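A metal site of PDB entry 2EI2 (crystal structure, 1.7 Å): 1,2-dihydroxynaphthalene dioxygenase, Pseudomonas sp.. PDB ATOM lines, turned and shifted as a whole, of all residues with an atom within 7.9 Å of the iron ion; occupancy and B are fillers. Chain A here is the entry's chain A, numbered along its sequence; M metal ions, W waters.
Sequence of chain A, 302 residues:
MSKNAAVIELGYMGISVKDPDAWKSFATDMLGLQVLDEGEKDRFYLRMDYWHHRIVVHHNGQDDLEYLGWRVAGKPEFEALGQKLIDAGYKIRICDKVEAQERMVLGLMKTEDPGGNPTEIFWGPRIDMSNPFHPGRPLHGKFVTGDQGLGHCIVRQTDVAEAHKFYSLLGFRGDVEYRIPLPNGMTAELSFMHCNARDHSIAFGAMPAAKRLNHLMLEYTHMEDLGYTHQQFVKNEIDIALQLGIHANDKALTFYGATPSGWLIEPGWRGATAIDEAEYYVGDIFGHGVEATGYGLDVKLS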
ATOM      1  N   HIS A 152       7.431  25.950  30.144  1.00  0.00           N
ATOM      2  CA  HIS A 152       7.303  26.641  28.856  1.00  0.00           C
ATOM      3  C   HIS A 152       6.437  25.898  27.865  1.00  0.00           C
ATOM      4  O   HIS A 152       6.224  24.689  27.987  1.00  0.00           O
ATOM      5  CB  HIS A 152       8.678  27.004  28.245  1.00  0.00           C
ATOM      6  CG  HIS A 152       9.452  25.846  27.663  1.00  0.00           C
ATOM      7  ND1 HIS A 152      10.738  25.559  28.076  1.00  0.00           N
ATOM      8  CD2 HIS A 152       9.195  24.996  26.634  1.00  0.00           C
ATOM      9  CE1 HIS A 152      11.204  24.544  27.371  1.00  0.00           C
ATOM     10  NE2 HIS A 152      10.299  24.190  26.474  1.00  0.00           N
ATOM     11  N   CYS A 153       5.930  26.605  26.870  1.00  0.00           N
ATOM     12  CA  CYS A 153       5.191  25.933  25.779  1.00  0.00           C
ATOM     13  C   CYS A 153       5.618  26.439  24.410  1.00  0.00           C
ATOM     14  O   CYS A 153       6.055  27.589  24.265  1.00  0.00           O
ATOM     15  CB  CYS A 153       3.701  26.283  25.851  1.00  0.00           C
ATOM     16  SG  CYS A 153       2.745  25.801  27.299  1.00  0.00           S
ATOM     17  N   ILE A 154       5.475  25.597  23.406  1.00  0.00           N
ATOM     18  CA  ILE A 154       5.421  26.046  22.007  1.00  0.00           C
ATOM     19  C   ILE A 154       3.945  26.042  21.606  1.00  0.00           C
ATOM     20  O   ILE A 154       3.243  25.042  21.845  1.00  0.00           O
ATOM     21  CB  ILE A 154       6.245  25.149  21.068  1.00  0.00           C
ATOM     22  CG1 ILE A 154       7.766  25.426  21.242  1.00  0.00           C
ATOM     23  CG2 ILE A 154       5.827  25.407  19.611  1.00  0.00           C
ATOM     24  CD1 ILE A 154       8.642  24.727  20.202  1.00  0.00           C
ATOM     25  N   PHE A 192      12.178  32.030  20.304  1.00  0.00           N
ATOM     26  CA  PHE A 192      12.039  31.667  21.713  1.00  0.00           C
ATOM     27  C   PHE A 192      12.087  32.913  22.557  1.00  0.00           C
ATOM     28  O   PHE A 192      13.023  33.703  22.409  1.00  0.00           O
ATOM     29  CB  PHE A 192      13.198  30.748  22.135  1.00  0.00           C
ATOM     30  CG  PHE A 192      13.215  29.453  21.381  1.00  0.00           C
ATOM     31  CD1 PHE A 192      13.775  29.383  20.099  1.00  0.00           C
ATOM     32  CD2 PHE A 192      12.675  28.296  21.927  1.00  0.00           C
ATOM     33  CE1 PHE A 192      13.797  28.201  19.389  1.00  0.00           C
ATOM     34  CE2 PHE A 192      12.697  27.098  21.213  1.00  0.00           C
ATOM     35  CZ  PHE A 192      13.247  27.039  19.957  1.00  0.00           C
ATOM     36  N   HIS A 200      13.301  29.985  28.199  1.00  0.00           N
ATOM     37  CA  HIS A 200      12.153  30.591  27.515  1.00  0.00           C
ATOM     38  C   HIS A 200      10.843  30.162  28.189  1.00  0.00           C
ATOM     39  O   HIS A 200      10.823  29.150  28.923  1.00  0.00           O
ATOM     40  CB  HIS A 200      12.122  30.287  26.000  1.00  0.00           C
ATOM     41  CG  HIS A 200      12.139  28.817  25.641  1.00  0.00           C
ATOM     42  ND1 HIS A 200      13.282  28.042  25.676  1.00  0.00           N
ATOM     43  CD2 HIS A 200      11.157  28.004  25.177  1.00  0.00           C
ATOM     44  CE1 HIS A 200      12.999  26.823  25.252  1.00  0.00           C
ATOM     45  NE2 HIS A 200      11.719  26.773  24.940  1.00  0.00           N
ATOM     46  N   ALA A 203       7.391  29.913  22.813  1.00  0.00           N
ATOM     47  CA  ALA A 203       8.167  29.770  21.581  1.00  0.00           C
ATOM     48  C   ALA A 203       7.238  29.400  20.454  1.00  0.00           C
ATOM     49  O   ALA A 203       6.125  28.932  20.687  1.00  0.00           O
ATOM     50  CB  ALA A 203       9.262  28.715  21.775  1.00  0.00           C
ATOM     51  N   ASN A 214       1.805  22.698  20.916  1.00  0.00           N
ATOM     52  CA  ASN A 214       2.749  21.693  20.420  1.00  0.00           C
ATOM     53  C   ASN A 214       3.320  20.846  21.553  1.00  0.00           C
ATOM     54  O   ASN A 214       3.260  19.603  21.516  1.00  0.00           O
ATOM     55  CB  ASN A 214       3.911  22.344  19.691  1.00  0.00           C
ATOM     56  CG  ASN A 214       5.005  21.335  19.375  1.00  0.00           C
ATOM     57  OD1 ASN A 214       6.023  21.274  20.066  1.00  0.00           O
ATOM     58  ND2 ASN A 214       4.766  20.492  18.361  1.00  0.00           N
ATOM     59  N   HIS A 215       3.897  21.533  22.536  1.00  0.00           N
ATOM     60  CA  HIS A 215       4.338  20.851  23.758  1.00  0.00           C
ATOM     61  C   HIS A 215       4.340  21.759  24.959  1.00  0.00           C
ATOM     62  O   HIS A 215       4.379  22.975  24.830  1.00  0.00           O
ATOM     63  CB  HIS A 215       5.732  20.188  23.593  1.00  0.00           C
ATOM     64  CG  HIS A 215       6.891  21.133  23.629  1.00  0.00           C
ATOM     65  ND1 HIS A 215       7.292  21.867  22.530  1.00  0.00           N
ATOM     66  CD2 HIS A 215       7.799  21.406  24.607  1.00  0.00           C
ATOM     67  CE1 HIS A 215       8.375  22.562  22.840  1.00  0.00           C
ATOM     68  NE2 HIS A 215       8.690  22.311  24.098  1.00  0.00           N
ATOM     69  N   LEU A 216       4.317  21.122  26.126  1.00  0.00           N
ATOM     70  CA  LEU A 216       4.522  21.777  27.426  1.00  0.00           C
ATOM     71  C   LEU A 216       5.744  21.134  28.083  1.00  0.00           C
ATOM     72  O   LEU A 216       5.820  19.913  28.175  1.00  0.00           O
ATOM     73  CB  LEU A 216       3.299  21.557  28.314  1.00  0.00           C
ATOM     74  CG  LEU A 216       3.460  21.867  29.815  1.00  0.00           C
ATOM     75  CD1 LEU A 216       3.734  23.363  30.071  1.00  0.00           C
ATOM     76  CD2 LEU A 216       2.265  21.362  30.653  1.00  0.00           C
ATOM     77  N   MET A 217       6.686  21.969  28.559  1.00  0.00           N
ATOM     78  CA  MET A 217       7.870  21.469  29.267  1.00  0.00           C
ATOM     79  C   MET A 217       7.693  21.706  30.760  1.00  0.00           C
ATOM     80  O   MET A 217       7.344  22.824  31.154  1.00  0.00           O
ATOM     81  CB  MET A 217       9.099  22.248  28.793  1.00  0.00           C
ATOM     82  CG  MET A 217      10.427  21.632  29.201  1.00  0.00           C
ATOM     83  SD  MET A 217      11.009  22.242  30.789  1.00  0.00           S
ATOM     84  CE  MET A 217      12.340  21.098  31.070  1.00  0.00           C
ATOM     85  N   LEU A 218       7.908  20.663  31.568  1.00  0.00           N
ATOM     86  CA  LEU A 218       7.906  20.769  33.041  1.00  0.00           C
ATOM     87  C   LEU A 218       9.270  20.306  33.545  1.00  0.00           C
ATOM     88  O   LEU A 218       9.769  19.276  33.075  1.00  0.00           O
ATOM     89  CB  LEU A 218       6.856  19.841  33.630  1.00  0.00           C
ATOM     90  CG  LEU A 218       5.404  20.161  33.202  1.00  0.00           C
ATOM     91  CD1 LEU A 218       4.440  19.171  33.860  1.00  0.00           C
ATOM     92  CD2 LEU A 218       5.038  21.628  33.566  1.00  0.00           C
ATOM     93  N   HIS A 247      18.867  20.427  24.033  1.00  0.00           N
ATOM     94  CA  HIS A 247      18.793  21.493  23.037  1.00  0.00           C
ATOM     95  C   HIS A 247      19.911  22.496  23.308  1.00  0.00           C
ATOM     96  O   HIS A 247      20.304  22.693  24.447  1.00  0.00           O
ATOM     97  CB  HIS A 247      17.469  22.258  23.103  1.00  0.00           C
ATOM     98  CG  HIS A 247      16.267  21.465  22.656  1.00  0.00           C
ATOM     99  ND1 HIS A 247      16.169  20.880  21.421  1.00  0.00           N
ATOM    100  CD2 HIS A 247      15.100  21.202  23.297  1.00  0.00           C
ATOM    101  CE1 HIS A 247      15.002  20.273  21.306  1.00  0.00           C
ATOM    102  NE2 HIS A 247      14.341  20.452  22.438  1.00  0.00           N
ATOM    103  N   ASN A 249      19.812  25.809  23.078  1.00  0.00           N
ATOM    104  CA  ASN A 249      19.447  27.029  23.811  1.00  0.00           C
ATOM    105  C   ASN A 249      19.193  26.813  25.288  1.00  0.00           C
ATOM    106  O   ASN A 249      19.924  27.375  26.115  1.00  0.00           O
ATOM    107  CB  ASN A 249      18.275  27.814  23.134  1.00  0.00           C
ATOM    108  CG  ASN A 249      17.062  26.938  22.798  1.00  0.00           C
ATOM    109  OD1 ASN A 249      17.031  25.750  23.067  1.00  0.00           O
ATOM    110  ND2 ASN A 249      16.040  27.550  22.167  1.00  0.00           N
ATOM    111  N   ASP A 250      18.209  25.985  25.653  1.00  0.00           N
ATOM    112  CA  ASP A 250      17.867  25.848  27.088  1.00  0.00           C
ATOM    113  C   ASP A 250      18.796  24.897  27.855  1.00  0.00           C
ATOM    114  O   ASP A 250      18.798  24.913  29.082  1.00  0.00           O
ATOM    115  CB  ASP A 250      16.387  25.443  27.281  1.00  0.00           C
ATOM    116  CG  ASP A 250      16.019  24.163  26.534  1.00  0.00           C
ATOM    117  OD1 ASP A 250      15.140  24.179  25.637  1.00  0.00           O
ATOM    118  OD2 ASP A 250      16.611  23.124  26.854  1.00  0.00           O
ATOM    119  N   THR A 254      16.236  16.555  28.356  1.00  0.00           N
ATOM    120  CA  THR A 254      14.786  16.365  28.227  1.00  0.00           C
ATOM    121  C   THR A 254      14.429  15.269  27.211  1.00  0.00           C
ATOM    122  O   THR A 254      15.267  14.874  26.382  1.00  0.00           O
ATOM    123  CB  THR A 254      14.053  17.662  27.735  1.00  0.00           C
ATOM    124  OG1 THR A 254      14.103  17.747  26.300  1.00  0.00           O
ATOM    125  CG2 THR A 254      14.561  18.957  28.388  1.00  0.00           C
ATOM    126  N   PHE A 255      13.178  14.791  27.252  1.00  0.00           N
ATOM    127  CA  PHE A 255      12.640  13.968  26.147  1.00  0.00           C
ATOM    128  C   PHE A 255      11.222  14.437  25.873  1.00  0.00           C
ATOM    129  O   PHE A 255      10.691  15.202  26.674  1.00  0.00           O
ATOM    130  CB  PHE A 255      12.694  12.460  26.423  1.00  0.00           C
ATOM    131  CG  PHE A 255      11.690  11.979  27.443  1.00  0.00           C
ATOM    132  CD1 PHE A 255      11.913  12.157  28.804  1.00  0.00           C
ATOM    133  CD2 PHE A 255      10.521  11.346  27.042  1.00  0.00           C
ATOM    134  CE1 PHE A 255      10.981  11.699  29.748  1.00  0.00           C
ATOM    135  CE2 PHE A 255       9.580  10.887  27.971  1.00  0.00           C
ATOM    136  CZ  PHE A 255       9.803  11.064  29.333  1.00  0.00           C
ATOM    137  N   TYR A 256      10.617  13.997  24.776  1.00  0.00           N
ATOM    138  CA  TYR A 256       9.249  14.433  24.464  1.00  0.00           C
ATOM    139  C   TYR A 256       8.349  13.201  24.356  1.00  0.00           C
ATOM    140  O   TYR A 256       8.657  12.302  23.569  1.00  0.00           O
ATOM    141  CB  TYR A 256       9.205  15.200  23.127  1.00  0.00           C
ATOM    142  CG  TYR A 256       9.869  16.557  23.098  1.00  0.00           C
ATOM    143  CD1 TYR A 256      11.266  16.703  23.194  1.00  0.00           C
ATOM    144  CD2 TYR A 256       9.106  17.709  22.933  1.00  0.00           C
ATOM    145  CE1 TYR A 256      11.864  17.979  23.166  1.00  0.00           C
ATOM    146  CE2 TYR A 256       9.690  18.956  22.878  1.00  0.00           C
ATOM    147  CZ  TYR A 256      11.075  19.100  22.981  1.00  0.00           C
ATOM    148  OH  TYR A 256      11.654  20.388  22.930  1.00  0.00           O
ATOM    149  N   ILE A 265       4.244  16.199  26.093  1.00  0.00           N
ATOM    150  CA  ILE A 265       4.853  16.709  27.334  1.00  0.00           C
ATOM    151  C   ILE A 265       6.354  16.542  27.222  1.00  0.00           C
ATOM    152  O   ILE A 265       6.816  15.558  26.651  1.00  0.00           O
ATOM    153  CB  ILE A 265       4.289  15.936  28.575  1.00  0.00           C
ATOM    154  CG1 ILE A 265       4.752  16.603  29.869  1.00  0.00           C
ATOM    155  CG2 ILE A 265       4.631  14.424  28.519  1.00  0.00           C
ATOM    156  CD1 ILE A 265       4.046  17.938  30.136  1.00  0.00           C
ATOM    157  N   GLU A 266       7.120  17.528  27.708  1.00  0.00           N
ATOM    158  CA  GLU A 266       8.568  17.453  27.642  1.00  0.00           C
ATOM    159  C   GLU A 266       9.105  17.518  29.082  1.00  0.00           C
ATOM    160  O   GLU A 266       9.356  18.599  29.598  1.00  0.00           O
ATOM    161  CB  GLU A 266       9.138  18.610  26.797  1.00  0.00           C
ATOM    162  CG  GLU A 266      10.673  18.638  26.740  1.00  0.00           C
ATOM    163  CD  GLU A 266      11.218  19.919  26.109  1.00  0.00           C
ATOM    164  OE1 GLU A 266      10.444  20.880  25.872  1.00  0.00           O
ATOM    165  OE2 GLU A 266      12.450  19.963  25.858  1.00  0.00           O
ATOM    166  N   HIS A 288      17.773  13.756  21.225  1.00  0.00           N
ATOM    167  CA  HIS A 288      16.482  14.152  20.672  1.00  0.00           C
ATOM    168  C   HIS A 288      16.237  13.530  19.276  1.00  0.00           C
ATOM    169  O   HIS A 288      15.642  14.177  18.402  1.00  0.00           O
ATOM    170  CB  HIS A 288      16.332  15.675  20.619  1.00  0.00           C
ATOM    171  CG  HIS A 288      16.122  16.331  21.956  1.00  0.00           C
ATOM    172  ND1 HIS A 288      16.590  17.593  22.243  1.00  0.00           N
ATOM    173  CD2 HIS A 288      15.471  15.910  23.074  1.00  0.00           C
ATOM    174  CE1 HIS A 288      16.259  17.919  23.485  1.00  0.00           C
ATOM    175  NE2 HIS A 288      15.559  16.928  24.006  1.00  0.00           N
ATOM    176  N   LEU A 297       7.004  17.253  15.331  1.00  0.00           N
ATOM    177  CA  LEU A 297       8.446  17.390  15.594  1.00  0.00           C
ATOM    178  C   LEU A 297       9.296  16.367  14.833  1.00  0.00           C
ATOM    179  O   LEU A 297      10.251  15.808  15.383  1.00  0.00           O
ATOM    180  CB  LEU A 297       8.728  17.327  17.091  1.00  0.00           C
ATOM    181  CG  LEU A 297       8.125  18.420  17.989  1.00  0.00           C
ATOM    182  CD1 LEU A 297       8.574  18.258  19.438  1.00  0.00           C
ATOM    183  CD2 LEU A 297       8.476  19.814  17.493  1.00  0.00           C
HETATM  184 FE    FE M   1      10.686  22.670  24.928  1.00  0.00          FE
HETATM  185  O   HOH W   1      11.097  24.190  23.611  1.00  0.00           O
HETATM  186  O   HOH W   2      12.821  22.511  25.470  1.00  0.00           O
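NE2 of His 200 lies close to NE2 of His 152 (3.3 Å).
The side-chain hydroxyl (OG1) of Thr 254 sits at hydrogen-bond distance from the side-chain carboxylate (OE2) of Glu 266.
The backbone carbonyl oxygen of Leu 216 sits at hydrogen-bond distance from the backbone NH of Glu 266, at 2.8 Å.
The backbone carbonyl oxygen of His 215 is in hydrogen-bond range of the backbone NH of Ile 154 (3.2 Å).
The backbone carbonyl oxygen of Glu 266 sits at hydrogen-bond distance from the backbone NH of Leu 218 (3.2 Å).
The side-chain amide oxygen (OD1) of Asn 214 sits at hydrogen-bond distance from a ring nitrogen (ND1) of His 215, at 2.8 Å.
The side-chain hydroxyl (OH) of Tyr 256 sits at hydrogen-bond distance from a ring nitrogen (NE2) of His 247, at 2.7 Å.
The side-chain hydroxyl (OH) of Tyr 256 sits at hydrogen-bond distance from the side-chain carboxylate (OE2) of Glu 266 (3.1 Å).
Tyr 256 touches the iron ion (OH to FE, 3.2 Å).
Within 4 Å of the iron ion: His 152, His 215, Tyr 256 and Glu 266.
OE1 of Glu 266 binds the iron ion.
Water W1 is bound to the iron ion.
The iron ion is bound by a ring nitrogen (NE2) of His 215.
The iron ion is bound by a ring nitrogen (NE2) of His 152, at 2.2 Å.
Water W2 is bound to the iron ion, 2.2 Å away.
Water W2 lies within hydrogen-bond range of the side-chain carboxylate of Glu 266 (2.6 Å) and the side-chain carboxylate of Asp 250 (2.9 Å).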
